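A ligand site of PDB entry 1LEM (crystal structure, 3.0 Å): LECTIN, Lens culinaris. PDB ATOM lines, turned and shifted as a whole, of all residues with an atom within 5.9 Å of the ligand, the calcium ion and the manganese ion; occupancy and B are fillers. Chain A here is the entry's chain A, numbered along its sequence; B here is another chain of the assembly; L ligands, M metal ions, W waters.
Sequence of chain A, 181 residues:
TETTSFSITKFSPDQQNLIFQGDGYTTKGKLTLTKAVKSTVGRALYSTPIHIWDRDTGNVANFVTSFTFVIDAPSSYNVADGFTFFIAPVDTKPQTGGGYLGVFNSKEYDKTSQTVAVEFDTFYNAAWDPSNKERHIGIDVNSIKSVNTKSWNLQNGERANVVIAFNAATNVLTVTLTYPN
An oxygen (O4) of the ligand is in hydrogen-bond range of the side-chain amide nitrogen (ND2) of Asn 125, at 3.1 Å.
OD2 of Asp 81 sits at hydrogen-bond distance from O6 of the ligand (2.8 Å).
The backbone NH (N) of Gly 99 is in hydrogen-bond range of an oxygen (O3) of the ligand (2.8 Å).
N of Ala 30 of chain B sits at hydrogen-bond distance from O6 of the ligand, 3.0 Å away.
N of Glu 31 of chain B is in hydrogen-bond range of O6 of the ligand, at 3.0 Å.
An oxygen (O6) of the ligand lies within hydrogen-bond range of the backbone carbonyl oxygen (O) of Glu 31 of chain B (3.2 Å).
An oxygen (O6) of the ligand lies close to the backbone NH of Gly 29 of chain B (3.4 Å).
The side-chain carboxylate (OD1) of Asp 129 sits close to the indole nitrogen (NE1) of Trp 128.
NE2 of His 136 lies close to OE2 of Glu 119, 3.5 Å away.
OE2 of Glu 119 is in hydrogen-bond range of OG of Ser 146, at 3.1 Å.
OD2 of Asp 81 lies within hydrogen-bond range of N of Gly 29 of chain B.
The backbone carbonyl oxygen (O) of Phe 32 of chain B sits at hydrogen-bond distance from the backbone NH (N) of Ala 80 (3.3 Å).
Ala 80 touches the ligand.
Gly 98 touches the ligand (C to O3, 3.7 Å).
Hydrophobic or aromatic side chains that line the ligand: Ala 80, Phe 123 and Ala 30 of chain B.
The nearest printed residue that does not touch the ligand is Thr 28 of chain B (4.5 Å).
Residues that only touch the calcium ion: Gly 99 and Trp 128.
Along chain A the residues within 4 Å of the calcium ion span positions 99 to 129.
Four residues have an atom within 4 Å of the manganese ion: Glu 119, Asp 121, Asp 129 and His 136.
The calcium ion is bound by the side-chain amide oxygen (OD1) of Asn 125 (2.1 Å), the side-chain carboxylate (OD2) of Asp 121 (2.4 Å), the side-chain carboxylate (OD2) of Asp 129 (2.5 Å), the backbone carbonyl oxygen (O) of Phe 123 (2.6 Å) and the side-chain carboxylate (OD1) of Asp 121 (2.7 Å).
The calcium ion has five donor atoms within binding distance.
The manganese ion is bound by OD1 of Asp 129 (2.1 Å), NE2 of His 136 (2.5 Å) and OD2 of Asp 121 (2.5 Å).
The manganese ion has three donor atoms within binding distance.
Slightly farther from the manganese ion lies OE2 of Glu 119 (2.8 Å).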
ATOM      1  N   ALA A  80     -16.768  -0.705 -30.520  1.00  0.00           N
ATOM      2  CA  ALA A  80     -17.220   0.672 -30.348  1.00  0.00           C
ATOM      3  C   ALA A  80     -17.495   1.178 -31.765  1.00  0.00           C
ATOM      4  O   ALA A  80     -16.828   0.671 -32.683  1.00  0.00           O
ATOM      5  CB  ALA A  80     -16.123   1.494 -29.660  1.00  0.00           C
ATOM      6  N   ASP A  81     -18.319   2.161 -32.114  1.00  0.00           N
ATOM      7  CA  ASP A  81     -19.075   2.905 -31.166  1.00  0.00           C
ATOM      8  C   ASP A  81     -20.563   2.975 -31.252  1.00  0.00           C
ATOM      9  O   ASP A  81     -21.234   3.429 -30.297  1.00  0.00           O
ATOM     10  CB  ASP A  81     -18.602   4.350 -31.252  1.00  0.00           C
ATOM     11  CG  ASP A  81     -17.733   4.755 -30.072  1.00  0.00           C
ATOM     12  OD1 ASP A  81     -18.247   4.881 -28.906  1.00  0.00           O
ATOM     13  OD2 ASP A  81     -16.474   4.974 -30.254  1.00  0.00           O
ATOM     14  N   GLY A  97     -18.306  13.109 -32.722  1.00  0.00           N
ATOM     15  CA  GLY A  97     -17.903  11.724 -32.881  1.00  0.00           C
ATOM     16  C   GLY A  97     -18.000  10.853 -31.641  1.00  0.00           C
ATOM     17  O   GLY A  97     -18.788  11.073 -30.712  1.00  0.00           O
ATOM     18  N   GLY A  98     -17.200   9.780 -31.698  1.00  0.00           N
ATOM     19  CA  GLY A  98     -17.123   8.783 -30.638  1.00  0.00           C
ATOM     20  C   GLY A  98     -18.476   8.408 -30.007  1.00  0.00           C
ATOM     21  O   GLY A  98     -19.432   8.157 -30.721  1.00  0.00           O
ATOM     22  N   GLY A  99     -18.719   8.509 -28.700  1.00  0.00           N
ATOM     23  CA  GLY A  99     -19.966   8.074 -28.089  1.00  0.00           C
ATOM     24  C   GLY A  99     -21.171   8.910 -28.461  1.00  0.00           C
ATOM     25  O   GLY A  99     -22.262   8.462 -28.063  1.00  0.00           O
ATOM     26  N   TYR A 100     -20.971  10.114 -29.106  1.00  0.00           N
ATOM     27  CA  TYR A 100     -22.022  11.037 -29.573  1.00  0.00           C
ATOM     28  C   TYR A 100     -22.572  10.643 -30.955  1.00  0.00           C
ATOM     29  O   TYR A 100     -23.574  11.186 -31.459  1.00  0.00           O
ATOM     30  CB  TYR A 100     -21.499  12.475 -29.644  1.00  0.00           C
ATOM     31  CG  TYR A 100     -21.330  13.097 -28.273  1.00  0.00           C
ATOM     32  CD1 TYR A 100     -22.445  13.339 -27.461  1.00  0.00           C
ATOM     33  CD2 TYR A 100     -20.066  13.411 -27.807  1.00  0.00           C
ATOM     34  CE1 TYR A 100     -22.289  13.889 -26.194  1.00  0.00           C
ATOM     35  CE2 TYR A 100     -19.896  13.961 -26.531  1.00  0.00           C
ATOM     36  CZ  TYR A 100     -21.002  14.209 -25.709  1.00  0.00           C
ATOM     37  OH  TYR A 100     -20.839  14.780 -24.432  1.00  0.00           O
ATOM     38  N   LEU A 101     -21.860   9.651 -31.564  1.00  0.00           N
ATOM     39  CA  LEU A 101     -22.253   8.872 -32.738  1.00  0.00           C
ATOM     40  C   LEU A 101     -22.409   9.709 -33.973  1.00  0.00           C
ATOM     41  O   LEU A 101     -23.218   9.357 -34.854  1.00  0.00           O
ATOM     42  CB  LEU A 101     -23.577   8.135 -32.432  1.00  0.00           C
ATOM     43  CG  LEU A 101     -23.623   7.132 -31.324  1.00  0.00           C
ATOM     44  CD1 LEU A 101     -24.964   6.451 -31.244  1.00  0.00           C
ATOM     45  CD2 LEU A 101     -22.577   6.085 -31.616  1.00  0.00           C
ATOM     46  N   GLU A 119     -30.701   4.564 -32.256  1.00  0.00           N
ATOM     47  CA  GLU A 119     -29.319   4.153 -32.182  1.00  0.00           C
ATOM     48  C   GLU A 119     -29.209   2.705 -31.753  1.00  0.00           C
ATOM     49  O   GLU A 119     -30.129   2.093 -31.175  1.00  0.00           O
ATOM     50  CB  GLU A 119     -28.595   5.057 -31.203  1.00  0.00           C
ATOM     51  CG  GLU A 119     -29.439   5.347 -29.935  1.00  0.00           C
ATOM     52  CD  GLU A 119     -28.714   5.808 -28.671  1.00  0.00           C
ATOM     53  OE1 GLU A 119     -28.118   6.900 -28.616  1.00  0.00           O
ATOM     54  OE2 GLU A 119     -28.804   5.068 -27.695  1.00  0.00           O
ATOM     55  N   ASP A 121     -26.284   1.196 -29.930  1.00  0.00           N
ATOM     56  CA  ASP A 121     -25.114   1.602 -29.131  1.00  0.00           C
ATOM     57  C   ASP A 121     -24.357   0.420 -28.579  1.00  0.00           C
ATOM     58  O   ASP A 121     -24.963  -0.380 -27.833  1.00  0.00           O
ATOM     59  CB  ASP A 121     -25.503   2.480 -27.959  1.00  0.00           C
ATOM     60  CG  ASP A 121     -24.320   3.233 -27.281  1.00  0.00           C
ATOM     61  OD1 ASP A 121     -23.133   2.966 -27.537  1.00  0.00           O
ATOM     62  OD2 ASP A 121     -24.610   4.153 -26.524  1.00  0.00           O
ATOM     63  N   THR A 122     -23.057   0.405 -28.878  1.00  0.00           N
ATOM     64  CA  THR A 122     -22.239  -0.767 -28.580  1.00  0.00           C
ATOM     65  C   THR A 122     -21.230  -0.524 -27.489  1.00  0.00           C
ATOM     66  O   THR A 122     -20.389  -1.371 -27.164  1.00  0.00           O
ATOM     67  CB  THR A 122     -21.402  -1.341 -29.845  1.00  0.00           C
ATOM     68  OG1 THR A 122     -20.667  -0.289 -30.495  1.00  0.00           O
ATOM     69  CG2 THR A 122     -22.308  -2.071 -30.821  1.00  0.00           C
ATOM     70  N   PHE A 123     -21.352   0.650 -26.899  1.00  0.00           N
ATOM     71  CA  PHE A 123     -20.362   1.063 -25.927  1.00  0.00           C
ATOM     72  C   PHE A 123     -20.942   2.041 -24.927  1.00  0.00           C
ATOM     73  O   PHE A 123     -21.516   3.075 -25.339  1.00  0.00           O
ATOM     74  CB  PHE A 123     -19.281   1.643 -26.749  1.00  0.00           C
ATOM     75  CG  PHE A 123     -18.157   2.065 -25.895  1.00  0.00           C
ATOM     76  CD1 PHE A 123     -17.184   1.133 -25.644  1.00  0.00           C
ATOM     77  CD2 PHE A 123     -18.064   3.365 -25.443  1.00  0.00           C
ATOM     78  CE1 PHE A 123     -16.087   1.512 -24.902  1.00  0.00           C
ATOM     79  CE2 PHE A 123     -16.967   3.730 -24.702  1.00  0.00           C
ATOM     80  CZ  PHE A 123     -15.980   2.811 -24.441  1.00  0.00           C
ATOM     81  N   TYR A 124     -20.755   1.646 -23.618  1.00  0.00           N
ATOM     82  CA  TYR A 124     -21.257   2.425 -22.474  1.00  0.00           C
ATOM     83  C   TYR A 124     -20.400   3.656 -22.177  1.00  0.00           C
ATOM     84  O   TYR A 124     -19.197   3.653 -21.877  1.00  0.00           O
ATOM     85  CB  TYR A 124     -21.355   1.542 -21.134  1.00  0.00           C
ATOM     86  CG  TYR A 124     -21.826   2.181 -19.779  1.00  0.00           C
ATOM     87  CD1 TYR A 124     -23.175   2.452 -19.512  1.00  0.00           C
ATOM     88  CD2 TYR A 124     -20.901   2.519 -18.757  1.00  0.00           C
ATOM     89  CE1 TYR A 124     -23.582   3.001 -18.288  1.00  0.00           C
ATOM     90  CE2 TYR A 124     -21.301   3.061 -17.534  1.00  0.00           C
ATOM     91  CZ  TYR A 124     -22.646   3.328 -17.307  1.00  0.00           C
ATOM     92  OH  TYR A 124     -23.070   3.921 -16.119  1.00  0.00           O
ATOM     93  N   ASN A 125     -21.138   4.752 -22.244  1.00  0.00           N
ATOM     94  CA  ASN A 125     -20.602   6.041 -21.962  1.00  0.00           C
ATOM     95  C   ASN A 125     -21.381   6.255 -20.693  1.00  0.00           C
ATOM     96  O   ASN A 125     -22.616   6.332 -20.585  1.00  0.00           O
ATOM     97  CB  ASN A 125     -20.986   6.972 -23.066  1.00  0.00           C
ATOM     98  CG  ASN A 125     -20.271   6.639 -24.379  1.00  0.00           C
ATOM     99  OD1 ASN A 125     -20.751   5.986 -25.319  1.00  0.00           O
ATOM    100  ND2 ASN A 125     -19.057   7.165 -24.389  1.00  0.00           N
ATOM    101  N   TRP A 128     -24.131   8.928 -19.678  1.00  0.00           N
ATOM    102  CA  TRP A 128     -25.496   9.084 -20.219  1.00  0.00           C
ATOM    103  C   TRP A 128     -26.136   7.770 -20.596  1.00  0.00           C
ATOM    104  O   TRP A 128     -27.359   7.681 -20.790  1.00  0.00           O
ATOM    105  CB  TRP A 128     -25.544   9.983 -21.508  1.00  0.00           C
ATOM    106  CG  TRP A 128     -24.622   9.618 -22.696  1.00  0.00           C
ATOM    107  CD1 TRP A 128     -24.793   8.462 -23.426  1.00  0.00           C
ATOM    108  CD2 TRP A 128     -23.501  10.314 -23.092  1.00  0.00           C
ATOM    109  NE1 TRP A 128     -23.768   8.388 -24.252  1.00  0.00           N
ATOM    110  CE2 TRP A 128     -22.958   9.469 -24.071  1.00  0.00           C
ATOM    111  CE3 TRP A 128     -22.833  11.477 -22.776  1.00  0.00           C
ATOM    112  CZ2 TRP A 128     -21.783   9.780 -24.744  1.00  0.00           C
ATOM    113  CZ3 TRP A 128     -21.650  11.780 -23.450  1.00  0.00           C
ATOM    114  CH2 TRP A 128     -21.122  10.949 -24.428  1.00  0.00           C
ATOM    115  N   ASP A 129     -25.310   6.740 -20.772  1.00  0.00           N
ATOM    116  CA  ASP A 129     -25.852   5.484 -21.252  1.00  0.00           C
ATOM    117  C   ASP A 129     -26.401   4.756 -20.043  1.00  0.00           C
ATOM    118  O   ASP A 129     -25.901   5.003 -18.928  1.00  0.00           O
ATOM    119  CB  ASP A 129     -24.742   4.664 -21.997  1.00  0.00           C
ATOM    120  CG  ASP A 129     -24.536   5.013 -23.496  1.00  0.00           C
ATOM    121  OD1 ASP A 129     -25.462   5.482 -24.159  1.00  0.00           O
ATOM    122  OD2 ASP A 129     -23.447   4.824 -24.032  1.00  0.00           O
ATOM    123  N   PRO A 130     -27.411   3.881 -20.178  1.00  0.00           N
ATOM    124  CA  PRO A 130     -27.982   3.076 -19.103  1.00  0.00           C
ATOM    125  C   PRO A 130     -26.932   2.433 -18.227  1.00  0.00           C
ATOM    126  O   PRO A 130     -26.086   1.633 -18.683  1.00  0.00           O
ATOM    127  CB  PRO A 130     -28.811   1.970 -19.685  1.00  0.00           C
ATOM    128  CG  PRO A 130     -29.117   2.520 -21.037  1.00  0.00           C
ATOM    129  CD  PRO A 130     -27.841   3.247 -21.421  1.00  0.00           C
ATOM    130  N   HIS A 136     -27.595  -1.616 -26.344  1.00  0.00           N
ATOM    131  CA  HIS A 136     -28.983  -1.213 -26.408  1.00  0.00           C
ATOM    132  C   HIS A 136     -29.394  -0.506 -27.674  1.00  0.00           C
ATOM    133  O   HIS A 136     -28.545   0.117 -28.346  1.00  0.00           O
ATOM    134  CB  HIS A 136     -29.249  -0.327 -25.193  1.00  0.00           C
ATOM    135  CG  HIS A 136     -28.293   0.862 -25.126  1.00  0.00           C
ATOM    136  ND1 HIS A 136     -27.055   0.869 -24.627  1.00  0.00           N
ATOM    137  CD2 HIS A 136     -28.557   2.167 -25.574  1.00  0.00           C
ATOM    138  CE1 HIS A 136     -26.581   2.090 -24.757  1.00  0.00           C
ATOM    139  NE2 HIS A 136     -27.479   2.880 -25.323  1.00  0.00           N
ATOM    140  N   ILE A 144     -27.936  13.235 -26.929  1.00  0.00           N
ATOM    141  CA  ILE A 144     -27.373  11.890 -26.905  1.00  0.00           C
ATOM    142  C   ILE A 144     -27.904  10.937 -25.822  1.00  0.00           C
ATOM    143  O   ILE A 144     -27.585   9.743 -25.783  1.00  0.00           O
ATOM    144  CB  ILE A 144     -25.859  11.990 -26.800  1.00  0.00           C
ATOM    145  CG1 ILE A 144     -25.219  10.653 -27.233  1.00  0.00           C
ATOM    146  CG2 ILE A 144     -25.475  12.308 -25.381  1.00  0.00           C
ATOM    147  CD1 ILE A 144     -25.342  10.194 -28.708  1.00  0.00           C
ATOM    148  N   SER A 146     -30.784   8.786 -24.641  1.00  0.00           N
ATOM    149  CA  SER A 146     -32.045   8.261 -25.130  1.00  0.00           C
ATOM    150  C   SER A 146     -33.231   8.504 -24.223  1.00  0.00           C
ATOM    151  O   SER A 146     -33.155   8.354 -23.012  1.00  0.00           O
ATOM    152  CB  SER A 146     -32.004   6.766 -25.342  1.00  0.00           C
ATOM    153  OG  SER A 146     -30.677   6.363 -25.665  1.00  0.00           O
ATOM    154  N   THR A 149     -34.952   3.129 -24.084  1.00  0.00           N
ATOM    155  CA  THR A 149     -33.980   2.138 -24.519  1.00  0.00           C
ATOM    156  C   THR A 149     -34.540   0.707 -24.345  1.00  0.00           C
ATOM    157  O   THR A 149     -35.582   0.464 -23.687  1.00  0.00           O
ATOM    158  CB  THR A 149     -32.612   2.229 -23.732  1.00  0.00           C
ATOM    159  OG1 THR A 149     -33.033   2.099 -22.416  1.00  0.00           O
ATOM    160  CG2 THR A 149     -31.786   3.501 -23.772  1.00  0.00           C
ATOM    161  N   THR B  28     -16.322   5.541 -34.327  1.00  0.00           N
ATOM    162  CA  THR B  28     -15.442   4.743 -33.509  1.00  0.00           C
ATOM    163  C   THR B  28     -14.620   5.802 -32.729  1.00  0.00           C
ATOM    164  O   THR B  28     -14.603   7.031 -33.019  1.00  0.00           O
ATOM    165  CB  THR B  28     -14.516   3.863 -34.386  1.00  0.00           C
ATOM    166  OG1 THR B  28     -13.737   4.761 -35.169  1.00  0.00           O
ATOM    167  CG2 THR B  28     -15.262   2.897 -35.277  1.00  0.00           C
ATOM    168  N   GLY B  29     -13.918   5.286 -31.712  1.00  0.00           N
ATOM    169  CA  GLY B  29     -13.025   6.082 -30.901  1.00  0.00           C
ATOM    170  C   GLY B  29     -11.855   5.169 -30.552  1.00  0.00           C
ATOM    171  O   GLY B  29     -11.267   4.516 -31.423  1.00  0.00           O
ATOM    172  N   ALA B  30     -11.674   5.085 -29.224  1.00  0.00           N
ATOM    173  CA  ALA B  30     -10.601   4.322 -28.588  1.00  0.00           C
ATOM    174  C   ALA B  30     -10.768   2.886 -29.023  1.00  0.00           C
ATOM    175  O   ALA B  30      -9.846   2.207 -29.466  1.00  0.00           O
ATOM    176  CB  ALA B  30     -10.722   4.335 -27.083  1.00  0.00           C
ATOM    177  N   GLU B  31     -11.952   2.374 -28.773  1.00  0.00           N
ATOM    178  CA  GLU B  31     -12.264   1.077 -29.321  1.00  0.00           C
ATOM    179  C   GLU B  31     -12.880   1.314 -30.741  1.00  0.00           C
ATOM    180  O   GLU B  31     -13.179   2.458 -31.125  1.00  0.00           O
ATOM    181  CB  GLU B  31     -13.158   0.471 -28.252  1.00  0.00           C
ATOM    182  CG  GLU B  31     -12.517  -0.723 -27.633  1.00  0.00           C
ATOM    183  CD  GLU B  31     -12.965  -0.881 -26.207  1.00  0.00           C
ATOM    184  OE1 GLU B  31     -12.456  -0.091 -25.411  1.00  0.00           O
ATOM    185  OE2 GLU B  31     -13.806  -1.737 -25.910  1.00  0.00           O
ATOM    186  N   PHE B  32     -13.214   0.286 -31.543  1.00  0.00           N
ATOM    187  CA  PHE B  32     -13.774   0.442 -32.881  1.00  0.00           C
ATOM    188  C   PHE B  32     -14.459  -0.829 -33.393  1.00  0.00           C
ATOM    189  O   PHE B  32     -14.509  -1.817 -32.655  1.00  0.00           O
ATOM    190  CB  PHE B  32     -12.699   0.819 -33.865  1.00  0.00           C
ATOM    191  CG  PHE B  32     -11.442   0.001 -33.676  1.00  0.00           C
ATOM    192  CD1 PHE B  32     -11.479  -1.391 -33.636  1.00  0.00           C
ATOM    193  CD2 PHE B  32     -10.252   0.676 -33.465  1.00  0.00           C
ATOM    194  CE1 PHE B  32     -10.340  -2.122 -33.384  1.00  0.00           C
ATOM    195  CE2 PHE B  32      -9.113  -0.069 -33.214  1.00  0.00           C
ATOM    196  CZ  PHE B  32      -9.165  -1.447 -33.172  1.00  0.00           C
HETATM  197  C1  LIG L   1     -13.146   7.593 -26.617  1.00  0.00           C
HETATM  198  C2  LIG L   1     -14.222   8.665 -26.994  1.00  0.00           C
HETATM  199  C3  LIG L   1     -15.664   8.180 -26.554  1.00  0.00           C
HETATM  200  C4  LIG L   1     -15.959   6.824 -27.187  1.00  0.00           C
HETATM  201  C5  LIG L   1     -14.948   5.773 -26.725  1.00  0.00           C
HETATM  202  C6  LIG L   1     -15.130   4.323 -27.401  1.00  0.00           C
HETATM  203  O1  LIG L   1     -13.030   7.669 -25.155  1.00  0.00           O
HETATM  204  O2  LIG L   1     -13.931   9.845 -26.251  1.00  0.00           O
HETATM  205  O3  LIG L   1     -16.717   9.106 -26.841  1.00  0.00           O
HETATM  206  O4  LIG L   1     -17.251   6.444 -26.802  1.00  0.00           O
HETATM  207  O5  LIG L   1     -13.612   6.277 -27.035  1.00  0.00           O
HETATM  208  O6  LIG L   1     -14.397   4.098 -28.608  1.00  0.00           O
HETATM  209 CA    CA M   1     -22.465   5.256 -26.311  1.00  0.00          CA
HETATM  210 MN    MN M   2     -26.768   5.189 -25.796  1.00  0.00          MN
HETATM  211  O   HOH W   1     -28.855   5.996 -23.731  1.00  0.00           O
